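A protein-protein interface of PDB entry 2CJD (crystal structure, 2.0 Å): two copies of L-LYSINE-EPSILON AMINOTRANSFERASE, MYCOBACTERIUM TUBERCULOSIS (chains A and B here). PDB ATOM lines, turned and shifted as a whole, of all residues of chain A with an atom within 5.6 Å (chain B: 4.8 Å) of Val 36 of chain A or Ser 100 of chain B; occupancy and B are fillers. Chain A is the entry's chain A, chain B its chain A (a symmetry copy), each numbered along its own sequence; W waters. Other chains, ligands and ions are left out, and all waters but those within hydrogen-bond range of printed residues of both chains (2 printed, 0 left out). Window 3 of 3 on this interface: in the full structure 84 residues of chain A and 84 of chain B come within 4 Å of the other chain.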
ATOM      1  N   PRO A  17      33.400  25.790   5.334  1.00  0.00           N
ATOM      2  CA  PRO A  17      32.056  26.360   5.124  1.00  0.00           C
ATOM      3  C   PRO A  17      30.994  25.362   4.633  1.00  0.00           C
ATOM      4  O   PRO A  17      29.853  25.368   5.127  1.00  0.00           O
ATOM      5  CB  PRO A  17      32.305  27.469   4.095  1.00  0.00           C
ATOM      6  CG  PRO A  17      33.655  27.923   4.373  1.00  0.00           C
ATOM      7  CD  PRO A  17      34.445  26.693   4.809  1.00  0.00           C
ATOM      8  N   ASP A  18      31.367  24.496   3.687  1.00  0.00           N
ATOM      9  CA  ASP A  18      30.390  23.542   3.125  1.00  0.00           C
ATOM     10  C   ASP A  18      30.001  22.411   4.097  1.00  0.00           C
ATOM     11  O   ASP A  18      29.044  21.691   3.846  1.00  0.00           O
ATOM     12  CB  ASP A  18      30.896  22.964   1.786  1.00  0.00           C
ATOM     13  CG  ASP A  18      32.053  22.025   1.976  1.00  0.00           C
ATOM     14  OD1 ASP A  18      33.120  22.487   2.437  1.00  0.00           O
ATOM     15  OD2 ASP A  18      31.899  20.808   1.689  1.00  0.00           O
ATOM     16  N   VAL A  20      29.569  23.219   7.593  1.00  0.00           N
ATOM     17  CA  VAL A  20      29.001  23.871   8.766  1.00  0.00           C
ATOM     18  C   VAL A  20      27.635  23.288   9.129  1.00  0.00           C
ATOM     19  O   VAL A  20      27.419  22.937  10.283  1.00  0.00           O
ATOM     20  CB  VAL A  20      28.906  25.403   8.552  1.00  0.00           C
ATOM     21  CG1 VAL A  20      27.901  26.066   9.535  1.00  0.00           C
ATOM     22  CG2 VAL A  20      30.310  26.011   8.615  1.00  0.00           C
ATOM     23  N   HIS A  21      26.725  23.193   8.160  1.00  0.00           N
ATOM     24  CA  HIS A  21      25.364  22.742   8.435  1.00  0.00           C
ATOM     25  C   HIS A  21      25.313  21.277   8.898  1.00  0.00           C
ATOM     26  O   HIS A  21      24.497  20.936   9.760  1.00  0.00           O
ATOM     27  CB  HIS A  21      24.431  22.944   7.230  1.00  0.00           C
ATOM     28  CG  HIS A  21      24.153  24.376   6.918  1.00  0.00           C
ATOM     29  ND1 HIS A  21      22.919  24.959   7.122  1.00  0.00           N
ATOM     30  CD2 HIS A  21      24.954  25.350   6.423  1.00  0.00           C
ATOM     31  CE1 HIS A  21      22.969  26.226   6.752  1.00  0.00           C
ATOM     32  NE2 HIS A  21      24.196  26.491   6.339  1.00  0.00           N
ATOM     33  N   LEU A  24      26.682  21.193  12.657  1.00  0.00           N
ATOM     34  CA  LEU A  24      25.696  21.720  13.598  1.00  0.00           C
ATOM     35  C   LEU A  24      24.490  20.789  13.718  1.00  0.00           C
ATOM     36  O   LEU A  24      23.928  20.603  14.824  1.00  0.00           O
ATOM     37  CB  LEU A  24      25.245  23.127  13.178  1.00  0.00           C
ATOM     38  CG  LEU A  24      26.326  24.222  13.187  1.00  0.00           C
ATOM     39  CD1 LEU A  24      25.771  25.516  12.586  1.00  0.00           C
ATOM     40  CD2 LEU A  24      26.812  24.482  14.576  1.00  0.00           C
ATOM     41  N   ASP A  34      20.313  29.283   4.609  1.00  0.00           N
ATOM     42  CA  ASP A  34      21.132  28.310   3.852  1.00  0.00           C
ATOM     43  C   ASP A  34      22.543  28.790   3.586  1.00  0.00           C
ATOM     44  O   ASP A  34      23.325  28.080   2.927  1.00  0.00           O
ATOM     45  CB  ASP A  34      20.547  27.997   2.471  1.00  0.00           C
ATOM     46  CG  ASP A  34      19.244  27.291   2.541  1.00  0.00           C
ATOM     47  OD1 ASP A  34      18.975  26.566   3.536  1.00  0.00           O
ATOM     48  OD2 ASP A  34      18.470  27.465   1.570  1.00  0.00           O
ATOM     49  N   ILE A  35      22.887  29.977   4.069  1.00  0.00           N
ATOM     50  CA  ILE A  35      24.209  30.499   3.805  1.00  0.00           C
ATOM     51  C   ILE A  35      25.127  30.225   4.973  1.00  0.00           C
ATOM     52  O   ILE A  35      24.672  29.802   6.050  1.00  0.00           O
ATOM     53  CB  ILE A  35      24.179  32.011   3.461  1.00  0.00           C
ATOM     54  CG1 ILE A  35      23.620  32.831   4.639  1.00  0.00           C
ATOM     55  CG2 ILE A  35      23.424  32.230   2.109  1.00  0.00           C
ATOM     56  CD1 ILE A  35      23.961  34.297   4.583  1.00  0.00           C
ATOM     57  N   VAL A  36      26.415  30.459   4.757  1.00  0.00           N
ATOM     58  CA  VAL A  36      27.342  30.458   5.852  1.00  0.00           C
ATOM     59  C   VAL A  36      27.972  31.839   5.860  1.00  0.00           C
ATOM     60  O   VAL A  36      28.538  32.269   4.847  1.00  0.00           O
ATOM     61  CB  VAL A  36      28.399  29.336   5.739  1.00  0.00           C
ATOM     62  CG1 VAL A  36      29.458  29.456   6.867  1.00  0.00           C
ATOM     63  CG2 VAL A  36      27.723  27.956   5.787  1.00  0.00           C
ATOM     64  N   LEU A  37      27.879  32.530   6.997  1.00  0.00           N
ATOM     65  CA  LEU A  37      28.350  33.903   7.086  1.00  0.00           C
ATOM     66  C   LEU A  37      29.869  34.000   6.997  1.00  0.00           C
ATOM     67  O   LEU A  37      30.588  33.456   7.824  1.00  0.00           O
ATOM     68  CB  LEU A  37      27.938  34.559   8.420  1.00  0.00           C
ATOM     69  CG  LEU A  37      27.565  36.057   8.527  1.00  0.00           C
ATOM     70  CD1 LEU A  37      28.041  36.746   9.813  1.00  0.00           C
ATOM     71  CD2 LEU A  37      27.804  36.908   7.304  1.00  0.00           C
ATOM     72  N   ASP A  38      30.340  34.776   6.034  1.00  0.00           N
ATOM     73  CA  ASP A  38      31.731  35.147   5.982  1.00  0.00           C
ATOM     74  C   ASP A  38      31.955  36.372   6.885  1.00  0.00           C
ATOM     75  O   ASP A  38      31.543  37.468   6.531  1.00  0.00           O
ATOM     76  CB  ASP A  38      32.125  35.467   4.545  1.00  0.00           C
ATOM     77  CG  ASP A  38      33.625  35.634   4.375  1.00  0.00           C
ATOM     78  OD1 ASP A  38      34.302  36.343   5.173  1.00  0.00           O
ATOM     79  OD2 ASP A  38      34.131  35.032   3.422  1.00  0.00           O
ATOM     80  N   LEU A  39      32.646  36.173   8.008  1.00  0.00           N
ATOM     81  CA  LEU A  39      32.802  37.186   9.039  1.00  0.00           C
ATOM     82  C   LEU A  39      33.721  38.295   8.592  1.00  0.00           C
ATOM     83  O   LEU A  39      33.627  39.407   9.067  1.00  0.00           O
ATOM     84  CB  LEU A  39      33.332  36.553  10.346  1.00  0.00           C
ATOM     85  CG  LEU A  39      32.379  35.538  11.020  1.00  0.00           C
ATOM     86  CD1 LEU A  39      33.048  34.996  12.301  1.00  0.00           C
ATOM     87  CD2 LEU A  39      31.088  36.212  11.364  1.00  0.00           C
ATOM     88  N   VAL A  48      28.035  38.219   3.114  1.00  0.00           N
ATOM     89  CA  VAL A  48      28.686  37.385   2.101  1.00  0.00           C
ATOM     90  C   VAL A  48      28.493  35.922   2.510  1.00  0.00           C
ATOM     91  O   VAL A  48      28.751  35.559   3.666  1.00  0.00           O
ATOM     92  CB  VAL A  48      30.171  37.778   1.936  1.00  0.00           C
ATOM     93  CG1 VAL A  48      30.923  36.818   0.990  1.00  0.00           C
ATOM     94  CG2 VAL A  48      30.283  39.203   1.436  1.00  0.00           C
ATOM     95  N   ASP A  49      27.998  35.103   1.583  1.00  0.00           N
ATOM     96  CA  ASP A  49      27.908  33.676   1.779  1.00  0.00           C
ATOM     97  C   ASP A  49      29.285  33.063   1.536  1.00  0.00           C
ATOM     98  O   ASP A  49      29.779  33.090   0.422  1.00  0.00           O
ATOM     99  CB  ASP A  49      26.844  33.061   0.846  1.00  0.00           C
ATOM    100  CG  ASP A  49      26.828  31.504   0.894  1.00  0.00           C
ATOM    101  OD1 ASP A  49      27.209  30.888   1.920  1.00  0.00           O
ATOM    102  OD2 ASP A  49      26.408  30.893  -0.101  1.00  0.00           O
ATOM    103  N   ALA A  50      29.889  32.500   2.583  1.00  0.00           N
ATOM    104  CA  ALA A  50      31.199  31.861   2.466  1.00  0.00           C
ATOM    105  C   ALA A  50      31.226  30.671   1.492  1.00  0.00           C
ATOM    106  O   ALA A  50      32.291  30.357   0.977  1.00  0.00           O
ATOM    107  CB  ALA A  50      31.712  31.426   3.826  1.00  0.00           C
ATOM    108  N   ILE A  51      30.095  30.000   1.270  1.00  0.00           N
ATOM    109  CA  ILE A  51      30.026  28.850   0.352  1.00  0.00           C
ATOM    110  C   ILE A  51      30.163  29.293  -1.129  1.00  0.00           C
ATOM    111  O   ILE A  51      31.026  28.766  -1.843  1.00  0.00           O
ATOM    112  CB  ILE A  51      28.738  28.019   0.562  1.00  0.00           C
ATOM    113  CG1 ILE A  51      28.728  27.369   1.964  1.00  0.00           C
ATOM    114  CG2 ILE A  51      28.587  26.914  -0.515  1.00  0.00           C
ATOM    115  CD1 ILE A  51      27.348  26.921   2.383  1.00  0.00           C
ATOM    116  N   VAL B  98      21.826  32.632  11.616  1.00  0.00           N
ATOM    117  CA  VAL B  98      22.969  32.703  10.700  1.00  0.00           C
ATOM    118  C   VAL B  98      24.183  31.963  11.243  1.00  0.00           C
ATOM    119  O   VAL B  98      24.745  32.355  12.276  1.00  0.00           O
ATOM    120  CB  VAL B  98      23.408  34.173  10.427  1.00  0.00           C
ATOM    121  CG1 VAL B  98      24.194  34.219   9.128  1.00  0.00           C
ATOM    122  CG2 VAL B  98      22.207  35.064  10.317  1.00  0.00           C
ATOM    123  N   TYR B  99      24.599  30.919  10.533  1.00  0.00           N
ATOM    124  CA  TYR B  99      25.669  30.042  11.010  1.00  0.00           C
ATOM    125  C   TYR B  99      27.001  30.468  10.459  1.00  0.00           C
ATOM    126  O   TYR B  99      27.070  31.150   9.437  1.00  0.00           O
ATOM    127  CB  TYR B  99      25.377  28.587  10.627  1.00  0.00           C
ATOM    128  CG  TYR B  99      23.998  28.147  11.044  1.00  0.00           C
ATOM    129  CD1 TYR B  99      23.499  28.447  12.322  1.00  0.00           C
ATOM    130  CD2 TYR B  99      23.185  27.442  10.171  1.00  0.00           C
ATOM    131  CE1 TYR B  99      22.225  28.064  12.705  1.00  0.00           C
ATOM    132  CE2 TYR B  99      21.914  27.055  10.547  1.00  0.00           C
ATOM    133  CZ  TYR B  99      21.451  27.359  11.804  1.00  0.00           C
ATOM    134  OH  TYR B  99      20.199  26.947  12.148  1.00  0.00           O
ATOM    135  N   SER B 100      28.070  30.093  11.158  1.00  0.00           N
ATOM    136  CA  SER B 100      29.403  30.445  10.732  1.00  0.00           C
ATOM    137  C   SER B 100      30.325  29.287  11.043  1.00  0.00           C
ATOM    138  O   SER B 100      29.976  28.363  11.799  1.00  0.00           O
ATOM    139  CB  SER B 100      29.884  31.724  11.448  1.00  0.00           C
ATOM    140  OG  SER B 100      29.876  31.563  12.866  1.00  0.00           O
ATOM    141  N   VAL B 101      31.511  29.328  10.450  1.00  0.00           N
ATOM    142  CA  VAL B 101      32.547  28.331  10.745  1.00  0.00           C
ATOM    143  C   VAL B 101      32.980  28.427  12.225  1.00  0.00           C
ATOM    144  O   VAL B 101      33.156  27.400  12.896  1.00  0.00           O
ATOM    145  CB  VAL B 101      33.748  28.521   9.825  1.00  0.00           C
ATOM    146  CG1 VAL B 101      35.009  27.816  10.402  1.00  0.00           C
ATOM    147  CG2 VAL B 101      33.385  28.022   8.379  1.00  0.00           C
ATOM    148  N   ALA B 102      33.131  29.662  12.718  1.00  0.00           N
ATOM    149  CA  ALA B 102      33.491  29.925  14.115  1.00  0.00           C
ATOM    150  C   ALA B 102      32.528  29.227  15.093  1.00  0.00           C
ATOM    151  O   ALA B 102      32.953  28.579  16.061  1.00  0.00           O
ATOM    152  CB  ALA B 102      33.518  31.432  14.364  1.00  0.00           C
ATOM    153  N   MET B 103      31.237  29.354  14.818  1.00  0.00           N
ATOM    154  CA  MET B 103      30.216  28.695  15.595  1.00  0.00           C
ATOM    155  C   MET B 103      30.317  27.160  15.518  1.00  0.00           C
ATOM    156  O   MET B 103      30.269  26.503  16.548  1.00  0.00           O
ATOM    157  CB  MET B 103      28.819  29.176  15.184  1.00  0.00           C
ATOM    158  CG  MET B 103      27.692  28.432  15.879  1.00  0.00           C
ATOM    159  SD  MET B 103      26.111  28.939  15.187  1.00  0.00           S
ATOM    160  CE  MET B 103      24.978  27.915  16.145  1.00  0.00           C
ATOM    161  N   ALA B 104      30.449  26.611  14.303  1.00  0.00           N
ATOM    162  CA  ALA B 104      30.518  25.159  14.108  1.00  0.00           C
ATOM    163  C   ALA B 104      31.733  24.547  14.810  1.00  0.00           C
ATOM    164  O   ALA B 104      31.619  23.462  15.397  1.00  0.00           O
ATOM    165  CB  ALA B 104      30.518  24.790  12.612  1.00  0.00           C
ATOM    166  N   LEU B 335      28.704  35.049  20.018  1.00  0.00           N
ATOM    167  CA  LEU B 335      29.746  34.398  19.196  1.00  0.00           C
ATOM    168  C   LEU B 335      31.173  34.588  19.757  1.00  0.00           C
ATOM    169  O   LEU B 335      31.988  33.668  19.688  1.00  0.00           O
ATOM    170  CB  LEU B 335      29.703  34.887  17.750  1.00  0.00           C
ATOM    171  CG  LEU B 335      30.652  34.202  16.764  1.00  0.00           C
ATOM    172  CD1 LEU B 335      30.250  32.688  16.646  1.00  0.00           C
ATOM    173  CD2 LEU B 335      30.524  34.905  15.416  1.00  0.00           C
HETATM  174  O   HOH W   1      23.200  30.370   8.189  1.00  0.00           O
HETATM  175  O   HOH W   2      32.199  31.461   8.608  1.00  0.00           O
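Printed residues of chain B within 4 Å of Val 36 of chain A: Tyr 99 (3.7 Å) and Ser 100 (3.99 Å).
Of the printed residues of chain A, Ser 100 of chain B touches Val 20 (3.8 Å) and Val 36 (3.99 Å).
Printed residues of chain A within 4 Å of Ala 104 of chain B: Leu 24 (3.8 Å).
Of the printed residues of chain B, His 21 of chain A touches Tyr 99.
Of the printed residues of chain A, Tyr 99 of chain B touches Val 20, His 21, Leu 24, Val 36 and Leu 37.
Leu 39 of chain A touches none of the printed residues of chain B.
The nearest printed residue of chain A that does not touch Ser 100 of chain B is Leu 37 of chain A (4.1 Å).
The nearest printed residue of chain A that does not touch Val 101 of chain B is Val 36 of chain A (4.1 Å).
O of Tyr 99 of chain B sits at hydrogen-bond distance from N of Leu 37 of chain A (2.9 Å).
Val 101 of chain B touches Pro 17 of chain A (CG2 to N, 3.8 Å).
Val 20 of chain A touches Tyr 99 of chain B (CG1 to CB, 3.7 Å).
CG1 of Val 20 of chain A touches O of Ser 100 of chain B, at 3.8 Å.
Val 20 of chain A touches Val 101 of chain B (CG2 to CG2, 3.7 Å).
His 21 of chain A touches Tyr 99 of chain B.
Leu 24 of chain A touches Tyr 99 of chain B (CD1 to CG, 3.5 Å).
Ala 104 of chain B touches Leu 24 of chain A.
CA of Val 36 of chain A touches O of Tyr 99 of chain B, 3.7 Å away.
CG1 of Val 36 of chain A touches CA of Ser 100 of chain B, at 3.99 Å.
Val 98 of chain B touches Leu 37 of chain A.
No position is printed for both chains.
Water W1 lies within hydrogen-bond range of O of Ile 35 of chain A and N of Tyr 99 of chain B.
Water W2 lies within hydrogen-bond range of the backbone carbonyl oxygen of Leu 37 of chain A (2.7 Å) and the backbone NH of Val 101 of chain B (2.9 Å).
Of the 8 printed residues of chain B, 5 touch a printed residue of chain A.
Printed residues of chain B that touch a printed residue of chain A: Val 98, Tyr 99, Ser 100, Val 101 and Ala 104.
Of the 15 printed residues of chain A, 6 touch a printed residue of chain B.
Printed residues of chain A that touch a printed residue of chain B: Pro 17, Val 20, His 21, Leu 24, Val 36 and Leu 37.
Hydrophobic or aromatic side chains of chain A that line the printed part of chain B: Pro 17, Val 20, His 21, Leu 24, Val 36 and Leu 37.
Among the printed residues, 11 pairs touch across the chains.
The backbone carbonyl oxygen (O) of Ile 35 of chain A is in hydrogen-bond range of a ring nitrogen (NE2) of His 21 of chain A, at 3.4 Å.
The backbone NH of Val 36 of chain A sits at hydrogen-bond distance from the side-chain carboxylate of Asp 49 of chain A (3.0 Å).
O of Val 36 of chain A sits at hydrogen-bond distance from N of Ala 50 of chain A, 2.6 Å away.
The side-chain hydroxyl of Ser 100 of chain B is in hydrogen-bond range of the backbone NH of Met 103 of chain B (3.2 Å).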
